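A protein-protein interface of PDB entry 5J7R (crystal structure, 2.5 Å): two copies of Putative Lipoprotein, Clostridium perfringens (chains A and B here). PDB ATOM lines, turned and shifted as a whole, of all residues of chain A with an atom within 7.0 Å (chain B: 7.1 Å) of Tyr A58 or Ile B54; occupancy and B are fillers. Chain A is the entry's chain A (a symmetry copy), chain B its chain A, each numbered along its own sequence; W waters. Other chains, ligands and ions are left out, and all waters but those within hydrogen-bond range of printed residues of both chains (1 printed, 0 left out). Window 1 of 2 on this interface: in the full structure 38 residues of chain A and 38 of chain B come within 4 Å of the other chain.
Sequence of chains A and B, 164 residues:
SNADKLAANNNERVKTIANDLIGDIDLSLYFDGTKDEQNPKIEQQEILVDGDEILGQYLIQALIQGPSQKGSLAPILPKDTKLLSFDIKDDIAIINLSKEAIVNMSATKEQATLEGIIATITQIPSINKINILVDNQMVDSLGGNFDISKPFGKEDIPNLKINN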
ATOM      1  N   ILE A  22     -27.939   6.046  -1.169  1.00  0.00           N
ATOM      2  CA  ILE A  22     -28.266   5.172  -0.027  1.00  0.00           C
ATOM      3  C   ILE A  22     -27.720   5.723   1.310  1.00  0.00           C
ATOM      4  O   ILE A  22     -28.358   5.584   2.334  1.00  0.00           O
ATOM      5  CB  ILE A  22     -27.709   3.743  -0.206  1.00  0.00           C
ATOM      6  CG1 ILE A  22     -28.099   3.177  -1.585  1.00  0.00           C
ATOM      7  CG2 ILE A  22     -28.201   2.850   0.934  1.00  0.00           C
ATOM      8  CD1 ILE A  22     -27.442   1.856  -1.932  1.00  0.00           C
ATOM      9  N   VAL A  49     -21.122   0.778   6.774  1.00  0.00           N
ATOM     10  CA  VAL A  49     -21.299   0.425   5.388  1.00  0.00           C
ATOM     11  C   VAL A  49     -21.666   1.682   4.661  1.00  0.00           C
ATOM     12  O   VAL A  49     -22.675   2.280   4.959  1.00  0.00           O
ATOM     13  CB  VAL A  49     -22.470  -0.556   5.208  1.00  0.00           C
ATOM     14  CG1 VAL A  49     -22.673  -0.890   3.742  1.00  0.00           C
ATOM     15  CG2 VAL A  49     -22.243  -1.821   6.014  1.00  0.00           C
ATOM     16  N   GLY A  51     -23.202   3.058   1.679  1.00  0.00           N
ATOM     17  CA  GLY A  51     -24.083   2.584   0.604  1.00  0.00           C
ATOM     18  C   GLY A  51     -23.708   2.890  -0.825  1.00  0.00           C
ATOM     19  O   GLY A  51     -23.789   2.013  -1.687  1.00  0.00           O
ATOM     20  N   ASP A  52     -23.330   4.135  -1.090  1.00  0.00           N
ATOM     21  CA  ASP A  52     -22.916   4.532  -2.434  1.00  0.00           C
ATOM     22  C   ASP A  52     -21.674   3.754  -2.865  1.00  0.00           C
ATOM     23  O   ASP A  52     -21.548   3.443  -4.049  1.00  0.00           O
ATOM     24  CB  ASP A  52     -22.704   6.053  -2.533  1.00  0.00           C
ATOM     25  CG  ASP A  52     -24.012   6.840  -2.378  1.00  0.00           C
ATOM     26  OD1 ASP A  52     -25.073   6.216  -2.150  1.00  0.00           O
ATOM     27  OD2 ASP A  52     -23.979   8.091  -2.500  1.00  0.00           O
ATOM     28  N   GLU A  53     -20.761   3.433  -1.931  1.00  0.00           N
ATOM     29  CA  GLU A  53     -19.575   2.647  -2.294  1.00  0.00           C
ATOM     30  C   GLU A  53     -19.956   1.225  -2.598  1.00  0.00           C
ATOM     31  O   GLU A  53     -19.436   0.656  -3.552  1.00  0.00           O
ATOM     32  CB  GLU A  53     -18.482   2.675  -1.241  1.00  0.00           C
ATOM     33  CG  GLU A  53     -17.850   4.041  -1.086  1.00  0.00           C
ATOM     34  CD  GLU A  53     -16.630   4.047  -0.168  1.00  0.00           C
ATOM     35  OE1 GLU A  53     -15.833   5.020  -0.216  1.00  0.00           O
ATOM     36  OE2 GLU A  53     -16.451   3.075   0.591  1.00  0.00           O
ATOM     37  N   ILE A  54     -20.847   0.635  -1.804  1.00  0.00           N
ATOM     38  CA  ILE A  54     -21.244  -0.752  -2.111  1.00  0.00           C
ATOM     39  C   ILE A  54     -22.025  -0.819  -3.420  1.00  0.00           C
ATOM     40  O   ILE A  54     -21.861  -1.770  -4.144  1.00  0.00           O
ATOM     41  CB  ILE A  54     -21.890  -1.613  -0.994  1.00  0.00           C
ATOM     42  CG1 ILE A  54     -23.304  -1.194  -0.649  1.00  0.00           C
ATOM     43  CG2 ILE A  54     -20.962  -1.645   0.196  1.00  0.00           C
ATOM     44  CD1 ILE A  54     -23.980  -2.187   0.275  1.00  0.00           C
ATOM     45  N   LEU A  55     -22.858   0.182  -3.709  1.00  0.00           N
ATOM     46  CA  LEU A  55     -23.625   0.214  -4.959  1.00  0.00           C
ATOM     47  C   LEU A  55     -22.681   0.402  -6.143  1.00  0.00           C
ATOM     48  O   LEU A  55     -22.763  -0.333  -7.132  1.00  0.00           O
ATOM     49  CB  LEU A  55     -24.658   1.334  -4.943  1.00  0.00           C
ATOM     50  CG  LEU A  55     -25.549   1.462  -6.180  1.00  0.00           C
ATOM     51  CD1 LEU A  55     -26.347   0.189  -6.426  1.00  0.00           C
ATOM     52  CD2 LEU A  55     -26.481   2.642  -6.000  1.00  0.00           C
ATOM     53  N   GLY A  56     -21.789   1.380  -6.036  1.00  0.00           N
ATOM     54  CA  GLY A  56     -20.811   1.647  -7.081  1.00  0.00           C
ATOM     55  C   GLY A  56     -19.967   0.417  -7.349  1.00  0.00           C
ATOM     56  O   GLY A  56     -19.710   0.047  -8.494  1.00  0.00           O
ATOM     57  N   GLN A  57     -19.554  -0.233  -6.277  1.00  0.00           N
ATOM     58  CA  GLN A  57     -18.742  -1.430  -6.390  1.00  0.00           C
ATOM     59  C   GLN A  57     -19.503  -2.516  -7.147  1.00  0.00           C
ATOM     60  O   GLN A  57     -18.937  -3.195  -7.983  1.00  0.00           O
ATOM     61  CB  GLN A  57     -18.295  -1.887  -5.001  1.00  0.00           C
ATOM     62  CG  GLN A  57     -17.516  -3.174  -4.973  1.00  0.00           C
ATOM     63  CD  GLN A  57     -16.893  -3.442  -3.610  1.00  0.00           C
ATOM     64  OE1 GLN A  57     -16.427  -2.523  -2.927  1.00  0.00           O
ATOM     65  NE2 GLN A  57     -16.812  -4.711  -3.241  1.00  0.00           N
ATOM     66  N   TYR A  58     -20.787  -2.670  -6.836  1.00  0.00           N
ATOM     67  CA  TYR A  58     -21.627  -3.654  -7.489  1.00  0.00           C
ATOM     68  C   TYR A  58     -21.742  -3.342  -8.995  1.00  0.00           C
ATOM     69  O   TYR A  58     -21.612  -4.241  -9.826  1.00  0.00           O
ATOM     70  CB  TYR A  58     -23.016  -3.663  -6.847  1.00  0.00           C
ATOM     71  CG  TYR A  58     -23.928  -4.721  -7.378  1.00  0.00           C
ATOM     72  CD1 TYR A  58     -23.921  -6.003  -6.835  1.00  0.00           C
ATOM     73  CD2 TYR A  58     -24.794  -4.452  -8.426  1.00  0.00           C
ATOM     74  CE1 TYR A  58     -24.760  -6.990  -7.311  1.00  0.00           C
ATOM     75  CE2 TYR A  58     -25.637  -5.443  -8.921  1.00  0.00           C
ATOM     76  CZ  TYR A  58     -25.616  -6.701  -8.360  1.00  0.00           C
ATOM     77  OH  TYR A  58     -26.441  -7.680  -8.829  1.00  0.00           O
ATOM     78  N   LEU A  59     -21.981  -2.069  -9.321  1.00  0.00           N
ATOM     79  CA  LEU A  59     -22.074  -1.609 -10.714  1.00  0.00           C
ATOM     80  C   LEU A  59     -20.805  -1.906 -11.504  1.00  0.00           C
ATOM     81  O   LEU A  59     -20.893  -2.423 -12.621  1.00  0.00           O
ATOM     82  CB  LEU A  59     -22.399  -0.109 -10.792  1.00  0.00           C
ATOM     83  CG  LEU A  59     -23.780   0.316 -10.280  1.00  0.00           C
ATOM     84  CD1 LEU A  59     -23.913   1.833 -10.274  1.00  0.00           C
ATOM     85  CD2 LEU A  59     -24.869  -0.315 -11.121  1.00  0.00           C
ATOM     86  N   ILE A  60     -19.632  -1.578 -10.954  1.00  0.00           N
ATOM     87  CA  ILE A  60     -18.381  -1.863 -11.662  1.00  0.00           C
ATOM     88  C   ILE A  60     -18.224  -3.362 -11.854  1.00  0.00           C
ATOM     89  O   ILE A  60     -17.700  -3.808 -12.881  1.00  0.00           O
ATOM     90  CB  ILE A  60     -17.127  -1.303 -10.932  1.00  0.00           C
ATOM     91  CG1 ILE A  60     -17.199   0.219 -10.824  1.00  0.00           C
ATOM     92  CG2 ILE A  60     -15.834  -1.685 -11.661  1.00  0.00           C
ATOM     93  CD1 ILE A  60     -17.283   0.950 -12.150  1.00  0.00           C
ATOM     94  N   GLN A  61     -18.683  -4.135 -10.871  1.00  0.00           N
ATOM     95  CA  GLN A  61     -18.541  -5.597 -10.953  1.00  0.00           C
ATOM     96  C   GLN A  61     -19.424  -6.061 -12.066  1.00  0.00           C
ATOM     97  O   GLN A  61     -19.084  -6.982 -12.784  1.00  0.00           O
ATOM     98  CB  GLN A  61     -19.044  -6.323  -9.681  1.00  0.00           C
ATOM     99  CG  GLN A  61     -18.195  -7.535  -9.298  1.00  0.00           C
ATOM    100  CD  GLN A  61     -16.811  -7.213  -8.760  1.00  0.00           C
ATOM    101  OE1 GLN A  61     -15.822  -7.662  -9.332  1.00  0.00           O
ATOM    102  NE2 GLN A  61     -16.723  -6.439  -7.682  1.00  0.00           N
ATOM    103  N   ALA A  62     -20.596  -5.439 -12.165  1.00  0.00           N
ATOM    104  CA  ALA A  62     -21.563  -5.788 -13.196  1.00  0.00           C
ATOM    105  C   ALA A  62     -21.041  -5.470 -14.603  1.00  0.00           C
ATOM    106  O   ALA A  62     -21.299  -6.224 -15.534  1.00  0.00           O
ATOM    107  CB  ALA A  62     -22.897  -5.104 -12.943  1.00  0.00           C
ATOM    108  N   LEU A  63     -20.311  -4.372 -14.744  1.00  0.00           N
ATOM    109  CA  LEU A  63     -19.719  -3.998 -16.040  1.00  0.00           C
ATOM    110  C   LEU A  63     -18.656  -5.015 -16.454  1.00  0.00           C
ATOM    111  O   LEU A  63     -18.577  -5.383 -17.612  1.00  0.00           O
ATOM    112  CB  LEU A  63     -19.101  -2.584 -16.000  1.00  0.00           C
ATOM    113  CG  LEU A  63     -20.041  -1.405 -15.830  1.00  0.00           C
ATOM    114  CD1 LEU A  63     -19.257  -0.114 -15.690  1.00  0.00           C
ATOM    115  CD2 LEU A  63     -21.013  -1.299 -16.996  1.00  0.00           C
ATOM    116  N   ILE A  64     -17.846  -5.453 -15.497  1.00  0.00           N
ATOM    117  CA  ILE A  64     -16.791  -6.441 -15.750  1.00  0.00           C
ATOM    118  C   ILE A  64     -17.392  -7.779 -16.178  1.00  0.00           C
ATOM    119  O   ILE A  64     -16.834  -8.452 -17.028  1.00  0.00           O
ATOM    120  CB  ILE A  64     -15.892  -6.636 -14.515  1.00  0.00           C
ATOM    121  CG1 ILE A  64     -15.091  -5.355 -14.251  1.00  0.00           C
ATOM    122  CG2 ILE A  64     -14.915  -7.789 -14.736  1.00  0.00           C
ATOM    123  CD1 ILE A  64     -14.343  -5.345 -12.932  1.00  0.00           C
ATOM    124  N   GLN A  65     -18.512  -8.167 -15.580  1.00  0.00           N
ATOM    125  CA  GLN A  65     -19.176  -9.424 -15.957  1.00  0.00           C
ATOM    126  C   GLN A  65     -19.615  -9.396 -17.421  1.00  0.00           C
ATOM    127  O   GLN A  65     -19.746 -10.447 -18.040  1.00  0.00           O
ATOM    128  CB  GLN A  65     -20.366  -9.731 -15.046  1.00  0.00           C
ATOM    129  CG  GLN A  65     -19.958 -10.079 -13.620  1.00  0.00           C
ATOM    130  CD  GLN A  65     -21.148 -10.226 -12.680  1.00  0.00           C
ATOM    131  OE1 GLN A  65     -22.278 -10.392 -13.125  1.00  0.00           O
ATOM    132  NE2 GLN A  65     -20.892 -10.180 -11.367  1.00  0.00           N
ATOM    133  N   LEU A  83     -11.834  -6.271  -9.838  1.00  0.00           N
ATOM    134  CA  LEU A  83     -11.962  -5.036  -9.087  1.00  0.00           C
ATOM    135  C   LEU A  83     -11.206  -5.203  -7.757  1.00  0.00           C
ATOM    136  O   LEU A  83     -11.614  -5.982  -6.904  1.00  0.00           O
ATOM    137  CB  LEU A  83     -13.439  -4.720  -8.846  1.00  0.00           C
ATOM    138  CG  LEU A  83     -13.747  -3.442  -8.074  1.00  0.00           C
ATOM    139  CD1 LEU A  83     -13.198  -2.216  -8.768  1.00  0.00           C
ATOM    140  CD2 LEU A  83     -15.234  -3.312  -7.912  1.00  0.00           C
ATOM    141  N   PHE A  86     -12.906  -0.182  -4.483  1.00  0.00           N
ATOM    142  CA  PHE A  86     -13.722   0.911  -4.951  1.00  0.00           C
ATOM    143  C   PHE A  86     -13.949   1.846  -3.773  1.00  0.00           C
ATOM    144  O   PHE A  86     -14.423   1.409  -2.729  1.00  0.00           O
ATOM    145  CB  PHE A  86     -15.040   0.395  -5.510  1.00  0.00           C
ATOM    146  CG  PHE A  86     -15.911   1.476  -6.046  1.00  0.00           C
ATOM    147  CD1 PHE A  86     -15.735   1.974  -7.330  1.00  0.00           C
ATOM    148  CD2 PHE A  86     -16.895   2.019  -5.262  1.00  0.00           C
ATOM    149  CE1 PHE A  86     -16.554   2.995  -7.811  1.00  0.00           C
ATOM    150  CE2 PHE A  86     -17.700   3.042  -5.730  1.00  0.00           C
ATOM    151  CZ  PHE A  86     -17.535   3.532  -6.998  1.00  0.00           C
ATOM    152  N   ILE B  22     -32.847  -0.977   2.273  1.00  0.00           N
ATOM    153  CA  ILE B  22     -32.513  -0.110   1.127  1.00  0.00           C
ATOM    154  C   ILE B  22     -33.534  -0.238  -0.025  1.00  0.00           C
ATOM    155  O   ILE B  22     -33.836   0.737  -0.685  1.00  0.00           O
ATOM    156  CB  ILE B  22     -31.113  -0.418   0.549  1.00  0.00           C
ATOM    157  CG1 ILE B  22     -30.058  -0.445   1.670  1.00  0.00           C
ATOM    158  CG2 ILE B  22     -30.766   0.603  -0.534  1.00  0.00           C
ATOM    159  CD1 ILE B  22     -28.687  -0.925   1.233  1.00  0.00           C
ATOM    160  N   ILE B  25     -33.310  -0.751  -6.588  1.00  0.00           N
ATOM    161  CA  ILE B  25     -32.870   0.461  -7.291  1.00  0.00           C
ATOM    162  C   ILE B  25     -32.782   0.079  -8.770  1.00  0.00           C
ATOM    163  O   ILE B  25     -31.979  -0.754  -9.158  1.00  0.00           O
ATOM    164  CB  ILE B  25     -31.517   1.028  -6.809  1.00  0.00           C
ATOM    165  CG1 ILE B  25     -31.493   1.114  -5.276  1.00  0.00           C
ATOM    166  CG2 ILE B  25     -31.235   2.367  -7.499  1.00  0.00           C
ATOM    167  CD1 ILE B  25     -30.185   1.593  -4.692  1.00  0.00           C
ATOM    168  N   LEU B  29     -26.735  -0.165 -16.933  1.00  0.00           N
ATOM    169  CA  LEU B  29     -25.348  -0.486 -17.166  1.00  0.00           C
ATOM    170  C   LEU B  29     -25.125  -0.084 -18.605  1.00  0.00           C
ATOM    171  O   LEU B  29     -25.909  -0.465 -19.480  1.00  0.00           O
ATOM    172  CB  LEU B  29     -25.065  -1.972 -17.010  1.00  0.00           C
ATOM    173  CG  LEU B  29     -25.223  -2.546 -15.621  1.00  0.00           C
ATOM    174  CD1 LEU B  29     -25.014  -4.047 -15.706  1.00  0.00           C
ATOM    175  CD2 LEU B  29     -24.239  -1.911 -14.638  1.00  0.00           C
ATOM    176  N   ILE B  47     -30.462  -2.918 -14.936  1.00  0.00           N
ATOM    177  CA  ILE B  47     -30.057  -3.735 -13.786  1.00  0.00           C
ATOM    178  C   ILE B  47     -30.913  -3.326 -12.584  1.00  0.00           C
ATOM    179  O   ILE B  47     -30.995  -2.160 -12.256  1.00  0.00           O
ATOM    180  CB  ILE B  47     -28.519  -3.654 -13.536  1.00  0.00           C
ATOM    181  CG1 ILE B  47     -28.064  -4.604 -12.411  1.00  0.00           C
ATOM    182  CG2 ILE B  47     -28.043  -2.229 -13.260  1.00  0.00           C
ATOM    183  CD1 ILE B  47     -26.577  -4.893 -12.429  1.00  0.00           C
ATOM    184  N   LEU B  48     -31.647  -4.270 -11.998  1.00  0.00           N
ATOM    185  CA  LEU B  48     -32.448  -3.980 -10.852  1.00  0.00           C
ATOM    186  C   LEU B  48     -31.575  -4.415  -9.689  1.00  0.00           C
ATOM    187  O   LEU B  48     -31.417  -5.604  -9.409  1.00  0.00           O
ATOM    188  CB  LEU B  48     -33.778  -4.709 -10.911  1.00  0.00           C
ATOM    189  CG  LEU B  48     -34.674  -4.233  -9.769  1.00  0.00           C
ATOM    190  CD1 LEU B  48     -35.184  -2.811  -9.975  1.00  0.00           C
ATOM    191  CD2 LEU B  48     -35.844  -5.164  -9.682  1.00  0.00           C
ATOM    192  N   VAL B  49     -30.980  -3.426  -9.034  1.00  0.00           N
ATOM    193  CA  VAL B  49     -30.109  -3.690  -7.917  1.00  0.00           C
ATOM    194  C   VAL B  49     -30.982  -3.845  -6.709  1.00  0.00           C
ATOM    195  O   VAL B  49     -31.680  -2.925  -6.346  1.00  0.00           O
ATOM    196  CB  VAL B  49     -29.175  -2.499  -7.645  1.00  0.00           C
ATOM    197  CG1 VAL B  49     -28.289  -2.771  -6.443  1.00  0.00           C
ATOM    198  CG2 VAL B  49     -28.330  -2.185  -8.866  1.00  0.00           C
ATOM    199  N   ASP B  50     -30.936  -5.014  -6.102  1.00  0.00           N
ATOM    200  CA  ASP B  50     -31.695  -5.304  -4.892  1.00  0.00           C
ATOM    201  C   ASP B  50     -30.809  -4.899  -3.716  1.00  0.00           C
ATOM    202  O   ASP B  50     -29.890  -5.621  -3.392  1.00  0.00           O
ATOM    203  CB  ASP B  50     -32.038  -6.809  -4.909  1.00  0.00           C
ATOM    204  CG  ASP B  50     -32.789  -7.293  -3.700  1.00  0.00           C
ATOM    205  OD1 ASP B  50     -32.518  -6.897  -2.570  1.00  0.00           O
ATOM    206  OD2 ASP B  50     -33.597  -8.202  -3.866  1.00  0.00           O
ATOM    207  N   GLY B  51     -31.100  -3.752  -3.087  1.00  0.00           N
ATOM    208  CA  GLY B  51     -30.263  -3.237  -1.994  1.00  0.00           C
ATOM    209  C   GLY B  51     -29.961  -4.145  -0.827  1.00  0.00           C
ATOM    210  O   GLY B  51     -28.816  -4.214  -0.378  1.00  0.00           O
ATOM    211  N   ASP B  52     -30.984  -4.817  -0.313  1.00  0.00           N
ATOM    212  CA  ASP B  52     -30.799  -5.747   0.799  1.00  0.00           C
ATOM    213  C   ASP B  52     -29.875  -6.893   0.392  1.00  0.00           C
ATOM    214  O   ASP B  52     -29.114  -7.371   1.231  1.00  0.00           O
ATOM    215  CB  ASP B  52     -32.146  -6.258   1.338  1.00  0.00           C
ATOM    216  CG  ASP B  52     -32.970  -5.151   2.008  1.00  0.00           C
ATOM    217  OD1 ASP B  52     -32.522  -3.983   2.018  1.00  0.00           O
ATOM    218  OD2 ASP B  52     -34.067  -5.458   2.542  1.00  0.00           O
ATOM    219  N   GLU B  53     -29.926  -7.339  -0.878  1.00  0.00           N
ATOM    220  CA  GLU B  53     -29.024  -8.408  -1.323  1.00  0.00           C
ATOM    221  C   GLU B  53     -27.611  -7.903  -1.418  1.00  0.00           C
ATOM    222  O   GLU B  53     -26.693  -8.613  -1.021  1.00  0.00           O
ATOM    223  CB  GLU B  53     -29.437  -9.041  -2.639  1.00  0.00           C
ATOM    224  CG  GLU B  53     -30.730  -9.820  -2.539  1.00  0.00           C
ATOM    225  CD  GLU B  53     -31.064 -10.613  -3.799  1.00  0.00           C
ATOM    226  OE1 GLU B  53     -31.911 -11.541  -3.732  1.00  0.00           O
ATOM    227  OE2 GLU B  53     -30.471 -10.327  -4.858  1.00  0.00           O
ATOM    228  N   ILE B  54     -27.415  -6.695  -1.943  1.00  0.00           N
ATOM    229  CA  ILE B  54     -26.034  -6.183  -2.017  1.00  0.00           C
ATOM    230  C   ILE B  54     -25.474  -5.920  -0.623  1.00  0.00           C
ATOM    231  O   ILE B  54     -24.309  -6.150  -0.414  1.00  0.00           O
ATOM    232  CB  ILE B  54     -25.711  -5.035  -3.009  1.00  0.00           C
ATOM    233  CG1 ILE B  54     -26.277  -3.694  -2.587  1.00  0.00           C
ATOM    234  CG2 ILE B  54     -26.129  -5.457  -4.397  1.00  0.00           C
ATOM    235  CD1 ILE B  54     -25.757  -2.563  -3.452  1.00  0.00           C
ATOM    236  N   LEU B  55     -26.303  -5.444   0.309  1.00  0.00           N
ATOM    237  CA  LEU B  55     -25.856  -5.191   1.684  1.00  0.00           C
ATOM    238  C   LEU B  55     -25.525  -6.512   2.375  1.00  0.00           C
ATOM    239  O   LEU B  55     -24.461  -6.651   2.982  1.00  0.00           O
ATOM    240  CB  LEU B  55     -26.920  -4.448   2.480  1.00  0.00           C
ATOM    241  CG  LEU B  55     -26.572  -4.094   3.927  1.00  0.00           C
ATOM    242  CD1 LEU B  55     -25.332  -3.214   4.002  1.00  0.00           C
ATOM    243  CD2 LEU B  55     -27.753  -3.396   4.566  1.00  0.00           C
ATOM    244  N   GLY B  56     -26.437  -7.473   2.275  1.00  0.00           N
ATOM    245  CA  GLY B  56     -26.234  -8.790   2.863  1.00  0.00           C
ATOM    246  C   GLY B  56     -24.973  -9.429   2.315  1.00  0.00           C
ATOM    247  O   GLY B  56     -24.170 -10.002   3.050  1.00  0.00           O
ATOM    248  N   GLN B  57     -24.793  -9.307   1.013  1.00  0.00           N
ATOM    249  CA  GLN B  57     -23.626  -9.869   0.360  1.00  0.00           C
ATOM    250  C   GLN B  57     -22.353  -9.238   0.919  1.00  0.00           C
ATOM    251  O   GLN B  57     -21.379  -9.927   1.158  1.00  0.00           O
ATOM    252  CB  GLN B  57     -23.748  -9.700  -1.155  1.00  0.00           C
ATOM    253  CG  GLN B  57     -22.556 -10.164  -1.946  1.00  0.00           C
ATOM    254  CD  GLN B  57     -22.836 -10.203  -3.443  1.00  0.00           C
ATOM    255  OE1 GLN B  57     -23.936 -10.557  -3.880  1.00  0.00           O
ATOM    256  NE2 GLN B  57     -21.818  -9.910  -4.237  1.00  0.00           N
ATOM    257  N   TYR B  58     -22.375  -7.923   1.114  1.00  0.00           N
ATOM    258  CA  TYR B  58     -21.240  -7.202   1.652  1.00  0.00           C
ATOM    259  C   TYR B  58     -20.927  -7.689   3.081  1.00  0.00           C
ATOM    260  O   TYR B  58     -19.767  -7.937   3.413  1.00  0.00           O
ATOM    261  CB  TYR B  58     -21.530  -5.700   1.660  1.00  0.00           C
ATOM    262  CG  TYR B  58     -20.377  -4.856   2.098  1.00  0.00           C
ATOM    263  CD1 TYR B  58     -19.420  -4.432   1.181  1.00  0.00           C
ATOM    264  CD2 TYR B  58     -20.232  -4.484   3.425  1.00  0.00           C
ATOM    265  CE1 TYR B  58     -18.351  -3.648   1.568  1.00  0.00           C
ATOM    266  CE2 TYR B  58     -19.152  -3.704   3.829  1.00  0.00           C
ATOM    267  CZ  TYR B  58     -18.223  -3.290   2.900  1.00  0.00           C
ATOM    268  OH  TYR B  58     -17.164  -2.519   3.278  1.00  0.00           O
ATOM    269  N   LEU B  59     -21.970  -7.822   3.904  1.00  0.00           N
ATOM    270  CA  LEU B  59     -21.838  -8.317   5.282  1.00  0.00           C
ATOM    271  C   LEU B  59     -21.212  -9.704   5.338  1.00  0.00           C
ATOM    272  O   LEU B  59     -20.295  -9.924   6.134  1.00  0.00           O
ATOM    273  CB  LEU B  59     -23.192  -8.325   6.010  1.00  0.00           C
ATOM    274  CG  LEU B  59     -23.829  -6.957   6.280  1.00  0.00           C
ATOM    275  CD1 LEU B  59     -25.226  -7.114   6.867  1.00  0.00           C
ATOM    276  CD2 LEU B  59     -22.949  -6.140   7.202  1.00  0.00           C
ATOM    277  N   PHE B  86     -25.351 -14.770  -3.139  1.00  0.00           N
ATOM    278  CA  PHE B  86     -26.190 -14.391  -2.031  1.00  0.00           C
ATOM    279  C   PHE B  86     -27.524 -13.940  -2.604  1.00  0.00           C
ATOM    280  O   PHE B  86     -27.556 -13.053  -3.452  1.00  0.00           O
ATOM    281  CB  PHE B  86     -25.535 -13.286  -1.215  1.00  0.00           C
ATOM    282  CG  PHE B  86     -26.339 -12.880  -0.030  1.00  0.00           C
ATOM    283  CD1 PHE B  86     -26.277 -13.589   1.162  1.00  0.00           C
ATOM    284  CD2 PHE B  86     -27.180 -11.801  -0.107  1.00  0.00           C
ATOM    285  CE1 PHE B  86     -27.046 -13.199   2.258  1.00  0.00           C
ATOM    286  CE2 PHE B  86     -27.955 -11.420   0.973  1.00  0.00           C
ATOM    287  CZ  PHE B  86     -27.893 -12.112   2.153  1.00  0.00           C
ATOM    288  N   ILE B  88     -31.971 -13.378  -1.608  1.00  0.00           N
ATOM    289  CA  ILE B  88     -33.023 -13.280  -0.594  1.00  0.00           C
ATOM    290  C   ILE B  88     -34.359 -13.741  -1.180  1.00  0.00           C
ATOM    291  O   ILE B  88     -34.931 -13.073  -2.035  1.00  0.00           O
ATOM    292  CB  ILE B  88     -33.164 -11.835  -0.054  1.00  0.00           C
ATOM    293  CG1 ILE B  88     -31.882 -11.417   0.687  1.00  0.00           C
ATOM    294  CG2 ILE B  88     -34.350 -11.726   0.901  1.00  0.00           C
ATOM    295  CD1 ILE B  88     -31.847  -9.961   1.108  1.00  0.00           C
ATOM    296  N   ILE B 124     -30.685  -7.121   8.727  1.00  0.00           N
ATOM    297  CA  ILE B 124     -31.458  -6.691   7.564  1.00  0.00           C
ATOM    298  C   ILE B 124     -32.882  -7.135   7.921  1.00  0.00           C
ATOM    299  O   ILE B 124     -33.146  -8.334   7.940  1.00  0.00           O
ATOM    300  CB  ILE B 124     -30.934  -7.349   6.276  1.00  0.00           C
ATOM    301  CG1 ILE B 124     -29.484  -6.912   6.021  1.00  0.00           C
ATOM    302  CG2 ILE B 124     -31.806  -6.948   5.094  1.00  0.00           C
ATOM    303  CD1 ILE B 124     -28.803  -7.601   4.855  1.00  0.00           C
HETATM  304  O   HOH W   1     -29.224  -7.002  -7.139  1.00  0.00           O
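The backbone NH of Ile B22 sits at hydrogen-bond distance from the side-chain carboxylate of Asp B52 (3.0 Å).
N of Ile B25 lies within hydrogen-bond range of O of Val B49, 2.7 Å away.
The backbone NH (N) of Ile A22 is in hydrogen-bond range of the side-chain carboxylate (OD1) of Asp A52 (3.0 Å).
Printed residues of chain A that touch a printed residue of chain B: Ile A22, Val A49, Ile A54, Leu A55, Tyr A58, Leu A59 and Ala A62.
Hydrophobic or aromatic side chains of chain A that line the printed part of chain B: Ile A22, Val A49, Ile A54, Leu A55, Tyr A58, Leu A59 and Ala A62.
Of the 19 printed residues of chain B, 8 touch a printed residue of chain A.
Printed residues of chain B that touch a printed residue of chain A: Ile B22, Ile B25, Leu B29, Ile B47, Val B49, Ile B54, Leu B55 and Tyr B58.
Among the printed residues, 13 pairs touch across the chains.
Among the printed residues, no Asp or Glu carboxylate lies within 4 Å of a Lys or Arg side-chain nitrogen of the other chain.
Ile A22 touches its own counterpart, Ile B22.
Val A49 touches Leu B55, and with the chains exchanged Leu A55 touches Val B49.
Ile B54 touches its own counterpart, Ile A54.
Ile A54 touches Leu B55, and with the chains exchanged Leu A55 touches Ile B54.
Positions printed for both chains: 22, 49, 51, 52, 53, 54, 55, 56, 57, 58, 59 and 86.
Of the 13 pairs that touch across the chains among the printed residues, 8 have their exchanged pair printed and touching as well.
Ile A22 touches Ile B25.
Ile A54 touches Ile B54.
Ile A54 touches Leu B55 (CD1 to CA, 3.8 Å).
Tyr B58 touches Ile A54 (CD1 to CG2, 3.3 Å).
Leu A55 touches Val B49.
Ile B54 touches Leu A55.
Ile B54 touches Tyr A58.
CD2 of Leu A59 touches CD2 of Leu B29, at 3.9 Å.
CD1 of Leu B29 touches CB of Ala A62, at 3.6 Å.
CB of Ala A62 touches CD1 of Ile B47, at 3.7 Å.
Water W1 lies within hydrogen-bond range of the backbone NH (N) of Asp B50, the side-chain hydroxyl (OH) of Tyr A58 and the backbone carbonyl oxygen (O) of Leu B48.
Printed residues of chain A within 4 Å of Leu B29: Leu A59 and Ala A62.
Of the printed residues of chain A, Val B49 touches Leu A55.
The nearest residue of chain B that does not touch Tyr A58 is Val B49 (4.2 Å).
The nearest printed residue of chain A that does not touch Tyr B58 is Val A49 (4.2 Å).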
